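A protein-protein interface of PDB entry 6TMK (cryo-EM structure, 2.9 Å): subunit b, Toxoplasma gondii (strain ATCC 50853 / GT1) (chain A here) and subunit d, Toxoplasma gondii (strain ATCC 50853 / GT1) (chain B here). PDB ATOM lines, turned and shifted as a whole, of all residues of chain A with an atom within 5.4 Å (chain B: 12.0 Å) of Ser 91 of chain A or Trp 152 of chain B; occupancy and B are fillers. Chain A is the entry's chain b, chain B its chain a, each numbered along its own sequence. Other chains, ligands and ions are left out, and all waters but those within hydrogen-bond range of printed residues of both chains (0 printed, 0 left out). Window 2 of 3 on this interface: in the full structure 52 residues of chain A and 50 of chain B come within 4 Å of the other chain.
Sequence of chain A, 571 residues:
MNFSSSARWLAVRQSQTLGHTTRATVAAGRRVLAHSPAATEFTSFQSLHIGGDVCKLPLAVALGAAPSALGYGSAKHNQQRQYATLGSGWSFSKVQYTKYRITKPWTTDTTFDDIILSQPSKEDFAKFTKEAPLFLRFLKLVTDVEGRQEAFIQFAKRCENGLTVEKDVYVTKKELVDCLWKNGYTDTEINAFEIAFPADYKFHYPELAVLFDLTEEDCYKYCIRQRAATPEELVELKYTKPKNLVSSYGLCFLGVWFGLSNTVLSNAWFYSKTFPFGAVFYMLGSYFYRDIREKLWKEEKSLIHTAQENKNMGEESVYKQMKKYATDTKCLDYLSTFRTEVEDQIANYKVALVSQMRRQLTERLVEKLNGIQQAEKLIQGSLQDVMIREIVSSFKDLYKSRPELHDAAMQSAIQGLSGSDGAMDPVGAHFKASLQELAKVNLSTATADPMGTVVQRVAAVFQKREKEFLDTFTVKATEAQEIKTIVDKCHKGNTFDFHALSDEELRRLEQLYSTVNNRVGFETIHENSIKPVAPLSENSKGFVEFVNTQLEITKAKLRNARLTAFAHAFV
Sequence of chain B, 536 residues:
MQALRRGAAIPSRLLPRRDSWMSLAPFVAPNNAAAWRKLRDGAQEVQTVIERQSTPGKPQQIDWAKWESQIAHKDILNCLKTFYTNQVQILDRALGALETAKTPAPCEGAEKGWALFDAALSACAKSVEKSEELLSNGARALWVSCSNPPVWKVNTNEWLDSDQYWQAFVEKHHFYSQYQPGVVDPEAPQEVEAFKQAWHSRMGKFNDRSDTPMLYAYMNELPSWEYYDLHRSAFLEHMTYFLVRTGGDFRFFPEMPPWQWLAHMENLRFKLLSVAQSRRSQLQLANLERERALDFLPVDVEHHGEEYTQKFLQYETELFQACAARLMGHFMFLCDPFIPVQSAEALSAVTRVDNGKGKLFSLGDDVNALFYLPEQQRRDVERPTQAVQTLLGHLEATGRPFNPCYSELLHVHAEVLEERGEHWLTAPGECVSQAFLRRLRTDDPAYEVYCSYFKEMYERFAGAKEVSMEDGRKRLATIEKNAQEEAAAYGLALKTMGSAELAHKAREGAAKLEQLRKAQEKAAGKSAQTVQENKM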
ATOM      1  N   GLY A  89       0.548  13.959  20.031  1.00  0.00           N
ATOM      2  CA  GLY A  89       0.224  15.268  20.572  1.00  0.00           C
ATOM      3  C   GLY A  89      -0.332  15.197  21.984  1.00  0.00           C
ATOM      4  O   GLY A  89      -1.136  14.324  22.307  1.00  0.00           O
ATOM      5  N   TRP A  90       0.119  16.132  22.816  1.00  0.00           N
ATOM      6  CA  TRP A  90      -0.327  16.258  24.192  1.00  0.00           C
ATOM      7  C   TRP A  90      -1.437  17.285  24.354  1.00  0.00           C
ATOM      8  O   TRP A  90      -1.824  17.593  25.485  1.00  0.00           O
ATOM      9  CB  TRP A  90       0.854  16.630  25.085  1.00  0.00           C
ATOM     10  CG  TRP A  90       1.646  15.469  25.550  1.00  0.00           C
ATOM     11  CD1 TRP A  90       2.671  14.866  24.894  1.00  0.00           C
ATOM     12  CD2 TRP A  90       1.490  14.769  26.784  1.00  0.00           C
ATOM     13  NE1 TRP A  90       3.161  13.827  25.639  1.00  0.00           N
ATOM     14  CE2 TRP A  90       2.452  13.749  26.807  1.00  0.00           C
ATOM     15  CE3 TRP A  90       0.628  14.905  27.871  1.00  0.00           C
ATOM     16  CZ2 TRP A  90       2.576  12.870  27.871  1.00  0.00           C
ATOM     17  CZ3 TRP A  90       0.751  14.034  28.921  1.00  0.00           C
ATOM     18  CH2 TRP A  90       1.719  13.031  28.917  1.00  0.00           C
ATOM     19  N   SER A  91      -1.956  17.818  23.254  1.00  0.00           N
ATOM     20  CA  SER A  91      -2.956  18.878  23.302  1.00  0.00           C
ATOM     21  C   SER A  91      -4.318  18.257  23.572  1.00  0.00           C
ATOM     22  O   SER A  91      -4.837  17.498  22.749  1.00  0.00           O
ATOM     23  CB  SER A  91      -2.956  19.666  21.996  1.00  0.00           C
ATOM     24  OG  SER A  91      -3.597  20.918  22.153  1.00  0.00           O
ATOM     25  N   PHE A  92      -4.895  18.571  24.728  1.00  0.00           N
ATOM     26  CA  PHE A  92      -6.258  18.163  25.047  1.00  0.00           C
ATOM     27  C   PHE A  92      -7.211  18.965  24.177  1.00  0.00           C
ATOM     28  O   PHE A  92      -7.451  20.148  24.423  1.00  0.00           O
ATOM     29  CB  PHE A  92      -6.548  18.381  26.525  1.00  0.00           C
ATOM     30  CG  PHE A  92      -7.963  18.086  26.916  1.00  0.00           C
ATOM     31  CD1 PHE A  92      -8.397  16.781  27.046  1.00  0.00           C
ATOM     32  CD2 PHE A  92      -8.858  19.111  27.155  1.00  0.00           C
ATOM     33  CE1 PHE A  92      -9.692  16.504  27.410  1.00  0.00           C
ATOM     34  CE2 PHE A  92     -10.157  18.836  27.519  1.00  0.00           C
ATOM     35  CZ  PHE A  92     -10.574  17.534  27.648  1.00  0.00           C
ATOM     36  N   SER A  93      -7.759  18.323  23.152  1.00  0.00           N
ATOM     37  CA  SER A  93      -8.563  18.994  22.144  1.00  0.00           C
ATOM     38  C   SER A  93      -9.970  18.425  22.148  1.00  0.00           C
ATOM     39  O   SER A  93     -10.157  17.208  22.047  1.00  0.00           O
ATOM     40  CB  SER A  93      -7.943  18.846  20.756  1.00  0.00           C
ATOM     41  OG  SER A  93      -8.288  17.603  20.180  1.00  0.00           O
ATOM     42  N   GLU A 300      -9.992  16.070  33.960  1.00  0.00           N
ATOM     43  CA  GLU A 300      -9.140  15.519  32.914  1.00  0.00           C
ATOM     44  C   GLU A 300      -8.082  16.522  32.480  1.00  0.00           C
ATOM     45  O   GLU A 300      -6.914  16.161  32.283  1.00  0.00           O
ATOM     46  CB  GLU A 300      -9.998  15.091  31.727  1.00  0.00           C
ATOM     47  CG  GLU A 300      -9.217  14.470  30.600  1.00  0.00           C
ATOM     48  CD  GLU A 300      -9.995  13.396  29.869  1.00  0.00           C
ATOM     49  OE1 GLU A 300     -11.242  13.461  29.868  1.00  0.00           O
ATOM     50  OE2 GLU A 300      -9.357  12.487  29.296  1.00  0.00           O
ATOM     51  N   ILE A 304      -4.021  15.909  32.828  1.00  0.00           N
ATOM     52  CA  ILE A 304      -3.129  15.954  31.674  1.00  0.00           C
ATOM     53  C   ILE A 304      -2.027  16.980  31.898  1.00  0.00           C
ATOM     54  O   ILE A 304      -0.851  16.737  31.586  1.00  0.00           O
ATOM     55  CB  ILE A 304      -3.950  16.241  30.404  1.00  0.00           C
ATOM     56  CG1 ILE A 304      -4.784  15.017  30.045  1.00  0.00           C
ATOM     57  CG2 ILE A 304      -3.062  16.603  29.250  1.00  0.00           C
ATOM     58  CD1 ILE A 304      -6.024  15.323  29.291  1.00  0.00           C
ATOM     59  N   SER B 145      10.954   7.354  26.942  1.00  0.00           N
ATOM     60  CA  SER B 145       9.988   8.363  27.346  1.00  0.00           C
ATOM     61  C   SER B 145       9.581   9.243  26.173  1.00  0.00           C
ATOM     62  O   SER B 145       8.396   9.542  25.994  1.00  0.00           O
ATOM     63  CB  SER B 145      10.572   9.207  28.473  1.00  0.00           C
ATOM     64  OG  SER B 145       9.569   9.943  29.142  1.00  0.00           O
ATOM     65  N   ASN B 148       7.375   7.251  23.806  1.00  0.00           N
ATOM     66  CA  ASN B 148       6.105   6.761  24.293  1.00  0.00           C
ATOM     67  C   ASN B 148       4.970   7.564  23.674  1.00  0.00           C
ATOM     68  O   ASN B 148       5.179   8.674  23.181  1.00  0.00           O
ATOM     69  CB  ASN B 148       6.031   6.866  25.815  1.00  0.00           C
ATOM     70  CG  ASN B 148       6.841   5.809  26.520  1.00  0.00           C
ATOM     71  OD1 ASN B 148       7.559   6.104  27.472  1.00  0.00           O
ATOM     72  ND2 ASN B 148       6.725   4.573  26.075  1.00  0.00           N
ATOM     73  N   PRO B 149       3.756   7.027  23.682  1.00  0.00           N
ATOM     74  CA  PRO B 149       2.602   7.830  23.318  1.00  0.00           C
ATOM     75  C   PRO B 149       2.155   8.691  24.484  1.00  0.00           C
ATOM     76  O   PRO B 149       2.619   8.506  25.617  1.00  0.00           O
ATOM     77  CB  PRO B 149       1.536   6.782  22.961  1.00  0.00           C
ATOM     78  CG  PRO B 149       2.233   5.484  22.934  1.00  0.00           C
ATOM     79  CD  PRO B 149       3.388   5.614  23.838  1.00  0.00           C
ATOM     80  N   PRO B 150       1.260   9.644  24.247  1.00  0.00           N
ATOM     81  CA  PRO B 150       0.647  10.364  25.366  1.00  0.00           C
ATOM     82  C   PRO B 150      -0.190   9.436  26.231  1.00  0.00           C
ATOM     83  O   PRO B 150      -1.006   8.647  25.737  1.00  0.00           O
ATOM     84  CB  PRO B 150      -0.195  11.436  24.675  1.00  0.00           C
ATOM     85  CG  PRO B 150       0.525  11.678  23.418  1.00  0.00           C
ATOM     86  CD  PRO B 150       1.023  10.342  22.976  1.00  0.00           C
ATOM     87  N   VAL B 151       0.014   9.545  27.542  1.00  0.00           N
ATOM     88  CA  VAL B 151      -0.554   8.588  28.470  1.00  0.00           C
ATOM     89  C   VAL B 151      -2.063   8.748  28.564  1.00  0.00           C
ATOM     90  O   VAL B 151      -2.765   7.793  28.907  1.00  0.00           O
ATOM     91  CB  VAL B 151       0.141   8.743  29.835  1.00  0.00           C
ATOM     92  CG1 VAL B 151      -0.370   9.959  30.566  1.00  0.00           C
ATOM     93  CG2 VAL B 151      -0.016   7.491  30.658  1.00  0.00           C
ATOM     94  N   TRP B 152      -2.587   9.934  28.253  1.00  0.00           N
ATOM     95  CA  TRP B 152      -4.030  10.125  28.204  1.00  0.00           C
ATOM     96  C   TRP B 152      -4.638   9.606  26.911  1.00  0.00           C
ATOM     97  O   TRP B 152      -5.848   9.367  26.861  1.00  0.00           O
ATOM     98  CB  TRP B 152      -4.385  11.597  28.397  1.00  0.00           C
ATOM     99  CG  TRP B 152      -3.996  12.495  27.284  1.00  0.00           C
ATOM    100  CD1 TRP B 152      -2.820  13.160  27.145  1.00  0.00           C
ATOM    101  CD2 TRP B 152      -4.795  12.851  26.155  1.00  0.00           C
ATOM    102  NE1 TRP B 152      -2.829  13.899  25.993  1.00  0.00           N
ATOM    103  CE2 TRP B 152      -4.033  13.727  25.367  1.00  0.00           C
ATOM    104  CE3 TRP B 152      -6.079  12.510  25.732  1.00  0.00           C
ATOM    105  CZ2 TRP B 152      -4.511  14.265  24.184  1.00  0.00           C
ATOM    106  CZ3 TRP B 152      -6.549  13.044  24.558  1.00  0.00           C
ATOM    107  CH2 TRP B 152      -5.769  13.910  23.796  1.00  0.00           C
ATOM    108  N   LYS B 153      -3.827   9.423  25.872  1.00  0.00           N
ATOM    109  CA  LYS B 153      -4.276   8.712  24.686  1.00  0.00           C
ATOM    110  C   LYS B 153      -4.225   7.208  24.888  1.00  0.00           C
ATOM    111  O   LYS B 153      -4.997   6.474  24.265  1.00  0.00           O
ATOM    112  CB  LYS B 153      -3.413   9.093  23.489  1.00  0.00           C
ATOM    113  CG  LYS B 153      -3.792  10.381  22.823  1.00  0.00           C
ATOM    114  CD  LYS B 153      -2.814  10.712  21.727  1.00  0.00           C
ATOM    115  CE  LYS B 153      -3.352  11.751  20.781  1.00  0.00           C
ATOM    116  NZ  LYS B 153      -3.542  13.043  21.455  1.00  0.00           N
ATOM    117  N   VAL B 154      -3.313   6.736  25.732  1.00  0.00           N
ATOM    118  CA  VAL B 154      -3.147   5.303  25.926  1.00  0.00           C
ATOM    119  C   VAL B 154      -4.367   4.722  26.629  1.00  0.00           C
ATOM    120  O   VAL B 154      -4.966   5.354  27.509  1.00  0.00           O
ATOM    121  CB  VAL B 154      -1.862   5.016  26.714  1.00  0.00           C
ATOM    122  CG1 VAL B 154      -1.822   3.575  27.128  1.00  0.00           C
ATOM    123  CG2 VAL B 154      -0.668   5.352  25.874  1.00  0.00           C
ATOM    124  N   ASN B 155      -4.740   3.506  26.237  1.00  0.00           N
ATOM    125  CA  ASN B 155      -5.827   2.792  26.891  1.00  0.00           C
ATOM    126  C   ASN B 155      -5.422   2.398  28.305  1.00  0.00           C
ATOM    127  O   ASN B 155      -4.284   1.995  28.556  1.00  0.00           O
ATOM    128  CB  ASN B 155      -6.195   1.553  26.075  1.00  0.00           C
ATOM    129  CG  ASN B 155      -7.472   0.891  26.537  1.00  0.00           C
ATOM    130  OD1 ASN B 155      -7.468  -0.264  26.953  1.00  0.00           O
ATOM    131  ND2 ASN B 155      -8.576   1.607  26.434  1.00  0.00           N
ATOM    132  N   THR B 156      -6.373   2.502  29.229  1.00  0.00           N
ATOM    133  CA  THR B 156      -6.083   2.293  30.644  1.00  0.00           C
ATOM    134  C   THR B 156      -5.714   0.842  30.933  1.00  0.00           C
ATOM    135  O   THR B 156      -4.728   0.564  31.629  1.00  0.00           O
ATOM    136  CB  THR B 156      -7.287   2.733  31.470  1.00  0.00           C
ATOM    137  OG1 THR B 156      -7.760   3.991  30.983  1.00  0.00           O
ATOM    138  CG2 THR B 156      -6.925   2.892  32.907  1.00  0.00           C
ATOM    139  N   ASN B 157      -6.499  -0.102  30.415  1.00  0.00           N
ATOM    140  CA  ASN B 157      -6.222  -1.505  30.675  1.00  0.00           C
ATOM    141  C   ASN B 157      -4.919  -1.942  30.026  1.00  0.00           C
ATOM    142  O   ASN B 157      -4.219  -2.801  30.567  1.00  0.00           O
ATOM    143  CB  ASN B 157      -7.383  -2.361  30.181  1.00  0.00           C
ATOM    144  CG  ASN B 157      -7.587  -3.603  31.010  1.00  0.00           C
ATOM    145  OD1 ASN B 157      -7.258  -3.645  32.193  1.00  0.00           O
ATOM    146  ND2 ASN B 157      -8.136  -4.627  30.388  1.00  0.00           N
ATOM    147  N   GLU B 158      -4.562  -1.352  28.886  1.00  0.00           N
ATOM    148  CA  GLU B 158      -3.279  -1.662  28.272  1.00  0.00           C
ATOM    149  C   GLU B 158      -2.124  -1.169  29.134  1.00  0.00           C
ATOM    150  O   GLU B 158      -1.123  -1.873  29.307  1.00  0.00           O
ATOM    151  CB  GLU B 158      -3.211  -1.048  26.879  1.00  0.00           C
ATOM    152  CG  GLU B 158      -3.987  -1.805  25.831  1.00  0.00           C
ATOM    153  CD  GLU B 158      -3.922  -1.147  24.472  1.00  0.00           C
ATOM    154  OE1 GLU B 158      -3.476   0.015  24.399  1.00  0.00           O
ATOM    155  OE2 GLU B 158      -4.311  -1.792  23.477  1.00  0.00           O
ATOM    156  N   TRP B 159      -2.243   0.041  29.677  1.00  0.00           N
ATOM    157  CA  TRP B 159      -1.230   0.531  30.599  1.00  0.00           C
ATOM    158  C   TRP B 159      -1.083  -0.386  31.802  1.00  0.00           C
ATOM    159  O   TRP B 159       0.036  -0.693  32.228  1.00  0.00           O
ATOM    160  CB  TRP B 159      -1.567   1.949  31.052  1.00  0.00           C
ATOM    161  CG  TRP B 159      -0.691   2.409  32.151  1.00  0.00           C
ATOM    162  CD1 TRP B 159       0.621   2.727  32.058  1.00  0.00           C
ATOM    163  CD2 TRP B 159      -1.054   2.596  33.520  1.00  0.00           C
ATOM    164  NE1 TRP B 159       1.106   3.100  33.281  1.00  0.00           N
ATOM    165  CE2 TRP B 159       0.093   3.029  34.199  1.00  0.00           C
ATOM    166  CE3 TRP B 159      -2.239   2.441  34.238  1.00  0.00           C
ATOM    167  CZ2 TRP B 159       0.092   3.308  35.554  1.00  0.00           C
ATOM    168  CZ3 TRP B 159      -2.234   2.718  35.578  1.00  0.00           C
ATOM    169  CH2 TRP B 159      -1.081   3.147  36.223  1.00  0.00           C
ATOM    170  N   LEU B 160      -2.202  -0.832  32.368  1.00  0.00           N
ATOM    171  CA  LEU B 160      -2.124  -1.682  33.545  1.00  0.00           C
ATOM    172  C   LEU B 160      -1.598  -3.072  33.209  1.00  0.00           C
ATOM    173  O   LEU B 160      -0.999  -3.727  34.066  1.00  0.00           O
ATOM    174  CB  LEU B 160      -3.482  -1.765  34.221  1.00  0.00           C
ATOM    175  CG  LEU B 160      -3.396  -2.089  35.705  1.00  0.00           C
ATOM    176  CD1 LEU B 160      -3.014  -0.869  36.494  1.00  0.00           C
ATOM    177  CD2 LEU B 160      -4.703  -2.624  36.174  1.00  0.00           C
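Of the 14 printed residues of chain B, 3 touch a printed residue of chain A. Hydrophobic or aromatic side chains of chain B that line the printed part of chain A: Pro 150 and Trp 152. Along chain B the printed residues that touch a printed residue of chain A span positions 150 to 153. Of the 7 printed residues of chain A, 4 touch a printed residue of chain B. Hydrophobic or aromatic side chains of chain A that line the printed part of chain B: Trp 90 and Ile 304. Among the printed residues, no Asp or Glu carboxylate lies within 4 Å of a Lys or Arg side-chain nitrogen of the other chain.
The backbone carbonyl oxygen of Gly 89 of chain A sits at hydrogen-bond distance from the side-chain amino group of Lys 153 of chain B, at 2.9 Å.
Printed residues of chain B within 4 Å of Ser 91 of chain A: Trp 152 (3.6 Å). Trp 152 of chain B touches just these residues of chain A: Gly 89 (3.9 Å), Trp 90 (3.9 Å), Ser 91 (3.6 Å) and Ile 304 (3.8 Å). Gly 89 of chain A touches just these residues of chain B: Pro 150 (3.3 Å), Trp 152 (3.9 Å) and Lys 153 (2.9 Å). Trp 90 of chain A touches just one residue of chain B: Trp 152. No residue of chain B comes within 4 Å of Ser 93 of chain A. Ile 304 of chain A touches just one residue of chain B: Trp 152 (3.8 Å). Printed residues of chain A within 4 Å of Pro 150 of chain B: Gly 89 (3.3 Å). Printed residues of chain A within 4 Å of Lys 153 of chain B: Gly 89 (2.9 Å). Ser 145 of chain B touches none of the printed residues of chain A. The nearest residue of chain B that does not touch Ser 91 of chain A is Lys 153 of chain B (4.8 Å). The nearest residue of chain A that does not touch Trp 152 of chain B is Phe 92 of chain A (4.4 Å). The nearest printed residue of chain A that does not touch Lys 153 of chain B is Ser 91 of chain A (4.8 Å).
Gly 89 of chain A touches Pro 150 of chain B (O to CG, 3.3 Å). Trp 152 of chain B touches Gly 89 of chain A (CZ2 to O, 3.9 Å). NE1 of Trp 152 of chain B touches O of Trp 90 of chain A, 3.9 Å away. CZ2 of Trp 152 of chain B touches O of Ser 91 of chain A, at 3.6 Å. CG1 of Ile 304 of chain A touches CB of Trp 152 of chain B, at 3.8 Å.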
